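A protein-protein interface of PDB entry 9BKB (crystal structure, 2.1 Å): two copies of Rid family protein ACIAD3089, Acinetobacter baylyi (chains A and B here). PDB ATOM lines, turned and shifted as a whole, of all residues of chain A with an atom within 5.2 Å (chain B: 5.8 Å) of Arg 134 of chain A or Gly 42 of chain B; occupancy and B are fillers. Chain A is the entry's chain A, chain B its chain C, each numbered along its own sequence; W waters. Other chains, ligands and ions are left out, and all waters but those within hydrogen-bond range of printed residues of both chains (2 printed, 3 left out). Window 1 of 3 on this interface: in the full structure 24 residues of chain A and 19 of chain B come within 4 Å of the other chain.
OD1 of Asp 115 of chain A lies within hydrogen-bond range of N of Lys 27 of chain B. The backbone carbonyl oxygen (O) of His 132 of chain A sits at hydrogen-bond distance from the backbone NH (N) of Thr 29 of chain B (2.9 Å). N of Arg 134 of chain A sits at hydrogen-bond distance from OG of Ser 41 of chain B, 2.9 Å away. N of Gly 42 of chain B sits at hydrogen-bond distance from O of Arg 134 of chain A, 3.0 Å away. The side-chain hydroxyl of Thr 135 of chain A is in hydrogen-bond range of the backbone NH of Gly 42 of chain B (3.1 Å). The side-chain amide nitrogen (ND2) of Asn 151 of chain B sits at hydrogen-bond distance from the side-chain hydroxyl (OG1) of Thr 135 of chain A, at 2.9 Å. The backbone carbonyl oxygen (O) of Ser 136 of chain A lies close to the side-chain carboxylate (OE2) of Glu 149 of chain B (3.1 Å).
O of Met 97 of chain A lies within hydrogen-bond range of N of Thr 135 of chain A (3.2 Å). The backbone NH (N) of Val 99 of chain A sits at hydrogen-bond distance from the backbone carbonyl oxygen (O) of Thr 135 of chain A (2.8 Å). OG of Ser 111 of chain A is in hydrogen-bond range of NH2 of Arg 134 of chain A (3.1 Å). The backbone carbonyl oxygen (O) of Ala 114 of chain A sits at hydrogen-bond distance from the side-chain hydroxyl (OG) of Ser 118 of chain A. The side-chain hydroxyl of Ser 118 of chain A sits at hydrogen-bond distance from a ring nitrogen (NE2) of His 132 of chain A, 2.7 Å away. The side-chain amide nitrogen (NE2) of Gln 43 of chain B is in hydrogen-bond range of the backbone carbonyl oxygen (O) of Ser 41 of chain B (3.1 Å).
Among the printed residues, merely in contact across the chains: Asn 98 of chain A with Asn 151 of chain B (3.9 Å), Ser 118 of chain A with Lys 27 of chain B (3.4 Å), His 132 of chain A with Lys 27 of chain B (3.6 Å), His 132 of chain A with Tyr 28 of chain B (3.6 Å), Thr 133 of chain A with Thr 29 of chain B (3.4 Å), Thr 133 of chain A with Ser 41 of chain B (3.3 Å), Arg 134 of chain A with Lys 27 of chain B (3.8 Å), Arg 134 of chain A with Tyr 28 of chain B (3.5 Å) and Thr 135 of chain A with Glu 149 of chain B (3.2 Å).
Printed residues of chain B within 4 Å of Arg 134 of chain A: Lys 27 (3.8 Å), Tyr 28 (3.5 Å), Ser 41 (2.9 Å) and Gly 42 (3.0 Å). Printed residues of chain A within 4 Å of Glu 149 of chain B: Thr 135 (3.2 Å) and Ser 136 (3.1 Å). Printed residues of chain B within 4 Å of Thr 133 of chain A: Thr 29 and Ser 41. Printed residues of chain B within 4 Å of Ser 118 of chain A: Lys 27 (3.4 Å). Printed residues of chain B within 4 Å of Thr 135 of chain A: Gly 42, Glu 149 and Asn 151. Printed residues of chain A within 4 Å of Tyr 28 of chain B: His 132 and Arg 134. Ile 150 of chain B touches none of the printed residues of chain A. The nearest residue of chain B that does not touch Arg 134 of chain A is Thr 29 of chain B (4.5 Å). The nearest printed residue of chain A that does not touch Gly 42 of chain B is Ser 136 of chain A (6.1 Å). The nearest printed residue of chain B that does not touch Thr 133 of chain A is Met 40 of chain B (4.2 Å).
Of the 11 printed residues of chain B, 7 touch a printed residue of chain A. Hydrophobic or aromatic side chains of chain B that line the printed part of chain A: Tyr 28. Of the 12 printed residues of chain A, 8 touch a printed residue of chain B. Hydrophobic or aromatic side chains of chain A that line the printed part of chain B: His 132. Among the printed residues, 16 pairs touch across the chains.
No position is printed for both chains. Of the 16 pairs that touch across the chains among the printed residues, none has its exchanged pair printed and touching as well.
Water W1 lies within hydrogen-bond range of the backbone carbonyl oxygen (O) of Met 40 of chain B (2.7 Å) and the side-chain hydroxyl (OG1) of Thr 133 of chain A (2.8 Å). Water W2 bridges ND2 of Asn 151 of chain B (3.2 Å) and ND2 of Asn 98 of chain A (3.3 Å).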
ATOM      1  N   MET A  97      16.951   9.377  20.349  1.00  0.00           N
ATOM      2  CA  MET A  97      17.100  10.310  21.461  1.00  0.00           C
ATOM      3  C   MET A  97      17.858   9.616  22.578  1.00  0.00           C
ATOM      4  O   MET A  97      17.358   8.641  23.141  1.00  0.00           O
ATOM      5  CB  MET A  97      15.738  10.780  21.985  1.00  0.00           C
ATOM      6  CG  MET A  97      15.888  11.741  23.162  1.00  0.00           C
ATOM      7  SD  MET A  97      14.322  12.456  23.712  1.00  0.00           S
ATOM      8  CE  MET A  97      13.597  11.047  24.537  1.00  0.00           C
ATOM      9  N   ASN A  98      19.040  10.124  22.930  1.00  0.00           N
ATOM     10  CA  ASN A  98      19.827   9.537  24.018  1.00  0.00           C
ATOM     11  C   ASN A  98      19.779  10.469  25.231  1.00  0.00           C
ATOM     12  O   ASN A  98      20.142  11.642  25.127  1.00  0.00           O
ATOM     13  CB  ASN A  98      21.271   9.262  23.582  1.00  0.00           C
ATOM     14  CG  ASN A  98      21.354   8.272  22.410  1.00  0.00           C
ATOM     15  OD1 ASN A  98      20.803   7.177  22.471  1.00  0.00           O
ATOM     16  ND2 ASN A  98      22.027   8.673  21.332  1.00  0.00           N
ATOM     17  N   VAL A  99      19.331   9.935  26.370  1.00  0.00           N
ATOM     18  CA  VAL A  99      19.104  10.699  27.594  1.00  0.00           C
ATOM     19  C   VAL A  99      20.118  10.255  28.641  1.00  0.00           C
ATOM     20  O   VAL A  99      20.138   9.083  29.040  1.00  0.00           O
ATOM     21  CB  VAL A  99      17.669  10.511  28.121  1.00  0.00           C
ATOM     22  CG1 VAL A  99      17.430  11.379  29.365  1.00  0.00           C
ATOM     23  CG2 VAL A  99      16.639  10.809  27.021  1.00  0.00           C
ATOM     24  N   SER A 111      13.670   5.787  33.102  1.00  0.00           N
ATOM     25  CA  SER A 111      12.624   5.759  32.087  1.00  0.00           C
ATOM     26  C   SER A 111      11.613   6.880  32.316  1.00  0.00           C
ATOM     27  O   SER A 111      11.226   7.592  31.377  1.00  0.00           O
ATOM     28  CB  SER A 111      11.947   4.382  32.092  1.00  0.00           C
ATOM     29  OG  SER A 111      11.088   4.237  30.982  1.00  0.00           O
ATOM     30  N   ALA A 114      13.130  10.203  31.235  1.00  0.00           N
ATOM     31  CA  ALA A 114      13.125  10.344  29.781  1.00  0.00           C
ATOM     32  C   ALA A 114      11.722  10.607  29.238  1.00  0.00           C
ATOM     33  O   ALA A 114      11.565  11.219  28.166  1.00  0.00           O
ATOM     34  CB  ALA A 114      13.721   9.087  29.145  1.00  0.00           C
ATOM     35  N   ASP A 115      10.691  10.128  29.946  1.00  0.00           N
ATOM     36  CA  ASP A 115       9.319  10.414  29.524  1.00  0.00           C
ATOM     37  C   ASP A 115       9.043  11.918  29.453  1.00  0.00           C
ATOM     38  O   ASP A 115       8.225  12.356  28.644  1.00  0.00           O
ATOM     39  CB  ASP A 115       8.324   9.725  30.465  1.00  0.00           C
ATOM     40  CG  ASP A 115       8.283   8.216  30.266  1.00  0.00           C
ATOM     41  OD1 ASP A 115       8.768   7.731  29.214  1.00  0.00           O
ATOM     42  OD2 ASP A 115       7.751   7.511  31.145  1.00  0.00           O
ATOM     43  N   SER A 118      10.138  12.640  25.964  1.00  0.00           N
ATOM     44  CA  SER A 118       9.302  11.977  24.975  1.00  0.00           C
ATOM     45  C   SER A 118       7.945  12.664  24.869  1.00  0.00           C
ATOM     46  O   SER A 118       7.411  12.837  23.767  1.00  0.00           O
ATOM     47  CB  SER A 118       9.144  10.497  25.331  1.00  0.00           C
ATOM     48  OG  SER A 118      10.396   9.817  25.294  1.00  0.00           O
ATOM     49  N   HIS A 132      10.052   7.871  18.279  1.00  0.00           N
ATOM     50  CA  HIS A 132      11.504   7.926  18.396  1.00  0.00           C
ATOM     51  C   HIS A 132      11.962   6.676  19.128  1.00  0.00           C
ATOM     52  O   HIS A 132      11.208   6.101  19.920  1.00  0.00           O
ATOM     53  CB  HIS A 132      11.945   9.200  19.140  1.00  0.00           C
ATOM     54  CG  HIS A 132      11.295   9.359  20.481  1.00  0.00           C
ATOM     55  ND1 HIS A 132      10.011   9.835  20.630  1.00  0.00           N
ATOM     56  CD2 HIS A 132      11.728   9.054  21.728  1.00  0.00           C
ATOM     57  CE1 HIS A 132       9.686   9.831  21.911  1.00  0.00           C
ATOM     58  NE2 HIS A 132      10.713   9.370  22.600  1.00  0.00           N
ATOM     59  N   THR A 133      13.180   6.230  18.822  1.00  0.00           N
ATOM     60  CA  THR A 133      13.842   5.254  19.681  1.00  0.00           C
ATOM     61  C   THR A 133      14.566   6.026  20.789  1.00  0.00           C
ATOM     62  O   THR A 133      14.808   7.235  20.683  1.00  0.00           O
ATOM     63  CB  THR A 133      14.809   4.345  18.904  1.00  0.00           C
ATOM     64  OG1 THR A 133      15.947   5.100  18.459  1.00  0.00           O
ATOM     65  CG2 THR A 133      14.107   3.709  17.684  1.00  0.00           C
ATOM     66  N   ARG A 134      14.902   5.322  21.867  1.00  0.00           N
ATOM     67  CA  ARG A 134      15.413   6.021  23.032  1.00  0.00           C
ATOM     68  C   ARG A 134      16.347   5.130  23.842  1.00  0.00           C
ATOM     69  O   ARG A 134      16.179   3.913  23.894  1.00  0.00           O
ATOM     70  CB  ARG A 134      14.218   6.438  23.905  1.00  0.00           C
ATOM     71  CG  ARG A 134      14.474   7.447  24.968  1.00  0.00           C
ATOM     72  CD  ARG A 134      13.153   7.730  25.711  1.00  0.00           C
ATOM     73  NE  ARG A 134      12.821   6.740  26.731  1.00  0.00           N
ATOM     74  CZ  ARG A 134      11.731   6.794  27.486  1.00  0.00           C
ATOM     75  NH1 ARG A 134      10.840   7.766  27.348  1.00  0.00           N
ATOM     76  NH2 ARG A 134      11.538   5.864  28.416  1.00  0.00           N
ATOM     77  N   THR A 135      17.286   5.772  24.527  1.00  0.00           N
ATOM     78  CA  THR A 135      18.158   5.143  25.518  1.00  0.00           C
ATOM     79  C   THR A 135      18.258   6.106  26.698  1.00  0.00           C
ATOM     80  O   THR A 135      18.358   7.319  26.497  1.00  0.00           O
ATOM     81  CB  THR A 135      19.560   4.825  24.951  1.00  0.00           C
ATOM     82  OG1 THR A 135      19.462   3.833  23.915  1.00  0.00           O
ATOM     83  CG2 THR A 135      20.518   4.320  26.036  1.00  0.00           C
ATOM     84  N   SER A 136      18.188   5.576  27.921  1.00  0.00           N
ATOM     85  CA  SER A 136      18.219   6.405  29.125  1.00  0.00           C
ATOM     86  C   SER A 136      19.117   5.753  30.162  1.00  0.00           C
ATOM     87  O   SER A 136      18.842   4.631  30.604  1.00  0.00           O
ATOM     88  CB  SER A 136      16.802   6.601  29.681  1.00  0.00           C
ATOM     89  OG  SER A 136      16.771   7.708  30.557  1.00  0.00           O
ATOM     90  N   LYS B  27       7.676   5.619  26.932  1.00  0.00           N
ATOM     91  CA  LYS B  27       6.896   6.342  25.920  1.00  0.00           C
ATOM     92  C   LYS B  27       7.688   6.463  24.622  1.00  0.00           C
ATOM     93  O   LYS B  27       7.883   7.559  24.102  1.00  0.00           O
ATOM     94  CB  LYS B  27       6.510   7.749  26.444  1.00  0.00           C
ATOM     95  CG  LYS B  27       5.696   7.716  27.735  1.00  0.00           C
ATOM     96  CD  LYS B  27       4.708   8.863  27.869  1.00  0.00           C
ATOM     97  CE  LYS B  27       3.990   8.797  29.216  1.00  0.00           C
ATOM     98  NZ  LYS B  27       3.261   7.513  29.410  1.00  0.00           N
ATOM     99  N   TYR B  28       8.107   5.323  24.077  1.00  0.00           N
ATOM    100  CA  TYR B  28       9.007   5.315  22.932  1.00  0.00           C
ATOM    101  C   TYR B  28       8.796   4.040  22.127  1.00  0.00           C
ATOM    102  O   TYR B  28       8.074   3.130  22.536  1.00  0.00           O
ATOM    103  CB  TYR B  28      10.476   5.437  23.369  1.00  0.00           C
ATOM    104  CG  TYR B  28      10.931   4.242  24.179  1.00  0.00           C
ATOM    105  CD1 TYR B  28      10.628   4.139  25.540  1.00  0.00           C
ATOM    106  CD2 TYR B  28      11.641   3.209  23.591  1.00  0.00           C
ATOM    107  CE1 TYR B  28      11.031   3.044  26.281  1.00  0.00           C
ATOM    108  CE2 TYR B  28      12.040   2.110  24.319  1.00  0.00           C
ATOM    109  CZ  TYR B  28      11.735   2.034  25.664  1.00  0.00           C
ATOM    110  OH  TYR B  28      12.137   0.937  26.389  1.00  0.00           O
ATOM    111  N   THR B  29       9.488   3.973  20.994  1.00  0.00           N
ATOM    112  CA  THR B  29       9.385   2.878  20.046  1.00  0.00           C
ATOM    113  C   THR B  29      10.653   2.036  20.099  1.00  0.00           C
ATOM    114  O   THR B  29      11.756   2.577  20.207  1.00  0.00           O
ATOM    115  CB  THR B  29       9.163   3.444  18.645  1.00  0.00           C
ATOM    116  OG1 THR B  29       8.021   4.305  18.675  1.00  0.00           O
ATOM    117  CG2 THR B  29       8.958   2.331  17.620  1.00  0.00           C
ATOM    118  N   MET B  40      17.676   1.042  17.058  1.00  0.00           N
ATOM    119  CA  MET B  40      17.028   0.300  18.127  1.00  0.00           C
ATOM    120  C   MET B  40      17.259   0.976  19.467  1.00  0.00           C
ATOM    121  O   MET B  40      18.376   1.429  19.769  1.00  0.00           O
ATOM    122  CB  MET B  40      17.529  -1.141  18.173  1.00  0.00           C
ATOM    123  CG  MET B  40      17.519  -1.838  16.801  1.00  0.00           C
ATOM    124  SD  MET B  40      17.683  -3.643  16.885  1.00  0.00           S
ATOM    125  CE  MET B  40      16.324  -4.069  17.973  1.00  0.00           C
ATOM    126  N   SER B  41      16.196   1.022  20.263  1.00  0.00           N
ATOM    127  CA  SER B  41      16.249   1.555  21.615  1.00  0.00           C
ATOM    128  C   SER B  41      17.165   0.706  22.495  1.00  0.00           C
ATOM    129  O   SER B  41      17.445  -0.449  22.203  1.00  0.00           O
ATOM    130  CB  SER B  41      14.844   1.590  22.217  1.00  0.00           C
ATOM    131  OG  SER B  41      14.046   2.555  21.551  1.00  0.00           O
ATOM    132  N   GLY B  42      17.652   1.308  23.577  1.00  0.00           N
ATOM    133  CA  GLY B  42      18.442   0.546  24.532  1.00  0.00           C
ATOM    134  C   GLY B  42      17.629  -0.569  25.170  1.00  0.00           C
ATOM    135  O   GLY B  42      16.465  -0.391  25.536  1.00  0.00           O
ATOM    136  N   GLN B  43      18.247  -1.741  25.277  1.00  0.00           N
ATOM    137  CA  GLN B  43      17.609  -2.945  25.791  1.00  0.00           C
ATOM    138  C   GLN B  43      18.301  -3.346  27.085  1.00  0.00           C
ATOM    139  O   GLN B  43      19.518  -3.579  27.096  1.00  0.00           O
ATOM    140  CB  GLN B  43      17.700  -4.105  24.791  1.00  0.00           C
ATOM    141  CG  GLN B  43      17.158  -3.817  23.396  1.00  0.00           C
ATOM    142  CD  GLN B  43      15.681  -3.570  23.370  1.00  0.00           C
ATOM    143  OE1 GLN B  43      14.924  -4.168  24.131  1.00  0.00           O
ATOM    144  NE2 GLN B  43      15.258  -2.647  22.511  1.00  0.00           N
ATOM    145  N   ILE B  44      17.528  -3.440  28.161  1.00  0.00           N
ATOM    146  CA  ILE B  44      17.982  -4.030  29.420  1.00  0.00           C
ATOM    147  C   ILE B  44      17.606  -5.503  29.353  1.00  0.00           C
ATOM    148  O   ILE B  44      16.794  -5.876  28.494  1.00  0.00           O
ATOM    149  CB  ILE B  44      17.357  -3.331  30.641  1.00  0.00           C
ATOM    150  CG1 ILE B  44      15.829  -3.414  30.583  1.00  0.00           C
ATOM    151  CG2 ILE B  44      17.876  -1.899  30.794  1.00  0.00           C
ATOM    152  CD1 ILE B  44      15.154  -2.845  31.818  1.00  0.00           C
ATOM    153  N   GLU B 149      22.755  -2.278  29.723  1.00  0.00           N
ATOM    154  CA  GLU B 149      21.816  -1.792  28.715  1.00  0.00           C
ATOM    155  C   GLU B 149      22.546  -1.631  27.392  1.00  0.00           C
ATOM    156  O   GLU B 149      23.648  -1.080  27.357  1.00  0.00           O
ATOM    157  CB  GLU B 149      21.185  -0.456  29.132  1.00  0.00           C
ATOM    158  CG  GLU B 149      20.073   0.055  28.180  1.00  0.00           C
ATOM    159  CD  GLU B 149      19.423   1.354  28.657  1.00  0.00           C
ATOM    160  OE1 GLU B 149      19.004   2.160  27.799  1.00  0.00           O
ATOM    161  OE2 GLU B 149      19.410   1.626  29.876  1.00  0.00           O
ATOM    162  N   ILE B 150      21.948  -2.099  26.299  1.00  0.00           N
ATOM    163  CA  ILE B 150      22.637  -2.111  25.015  1.00  0.00           C
ATOM    164  C   ILE B 150      21.714  -1.560  23.932  1.00  0.00           C
ATOM    165  O   ILE B 150      20.560  -1.990  23.817  1.00  0.00           O
ATOM    166  CB  ILE B 150      23.099  -3.533  24.653  1.00  0.00           C
ATOM    167  CG1 ILE B 150      23.911  -4.142  25.800  1.00  0.00           C
ATOM    168  CG2 ILE B 150      23.947  -3.503  23.372  1.00  0.00           C
ATOM    169  CD1 ILE B 150      24.486  -5.524  25.502  1.00  0.00           C
ATOM    170  N   ASN B 151      22.223  -0.630  23.120  1.00  0.00           N
ATOM    171  CA  ASN B 151      21.456  -0.223  21.931  1.00  0.00           C
ATOM    172  C   ASN B 151      22.250  -0.518  20.657  1.00  0.00           C
ATOM    173  O   ASN B 151      23.440  -0.861  20.703  1.00  0.00           O
ATOM    174  CB  ASN B 151      21.005   1.256  21.996  1.00  0.00           C
ATOM    175  CG  ASN B 151      22.160   2.261  21.940  1.00  0.00           C
ATOM    176  OD1 ASN B 151      23.201   2.018  21.346  1.00  0.00           O
ATOM    177  ND2 ASN B 151      21.949   3.418  22.544  1.00  0.00           N
HETATM  178  O   HOH W   1      18.420   4.128  19.421  1.00  0.00           O
HETATM  179  O   HOH W   2      23.722   5.897  21.681  1.00  0.00           O
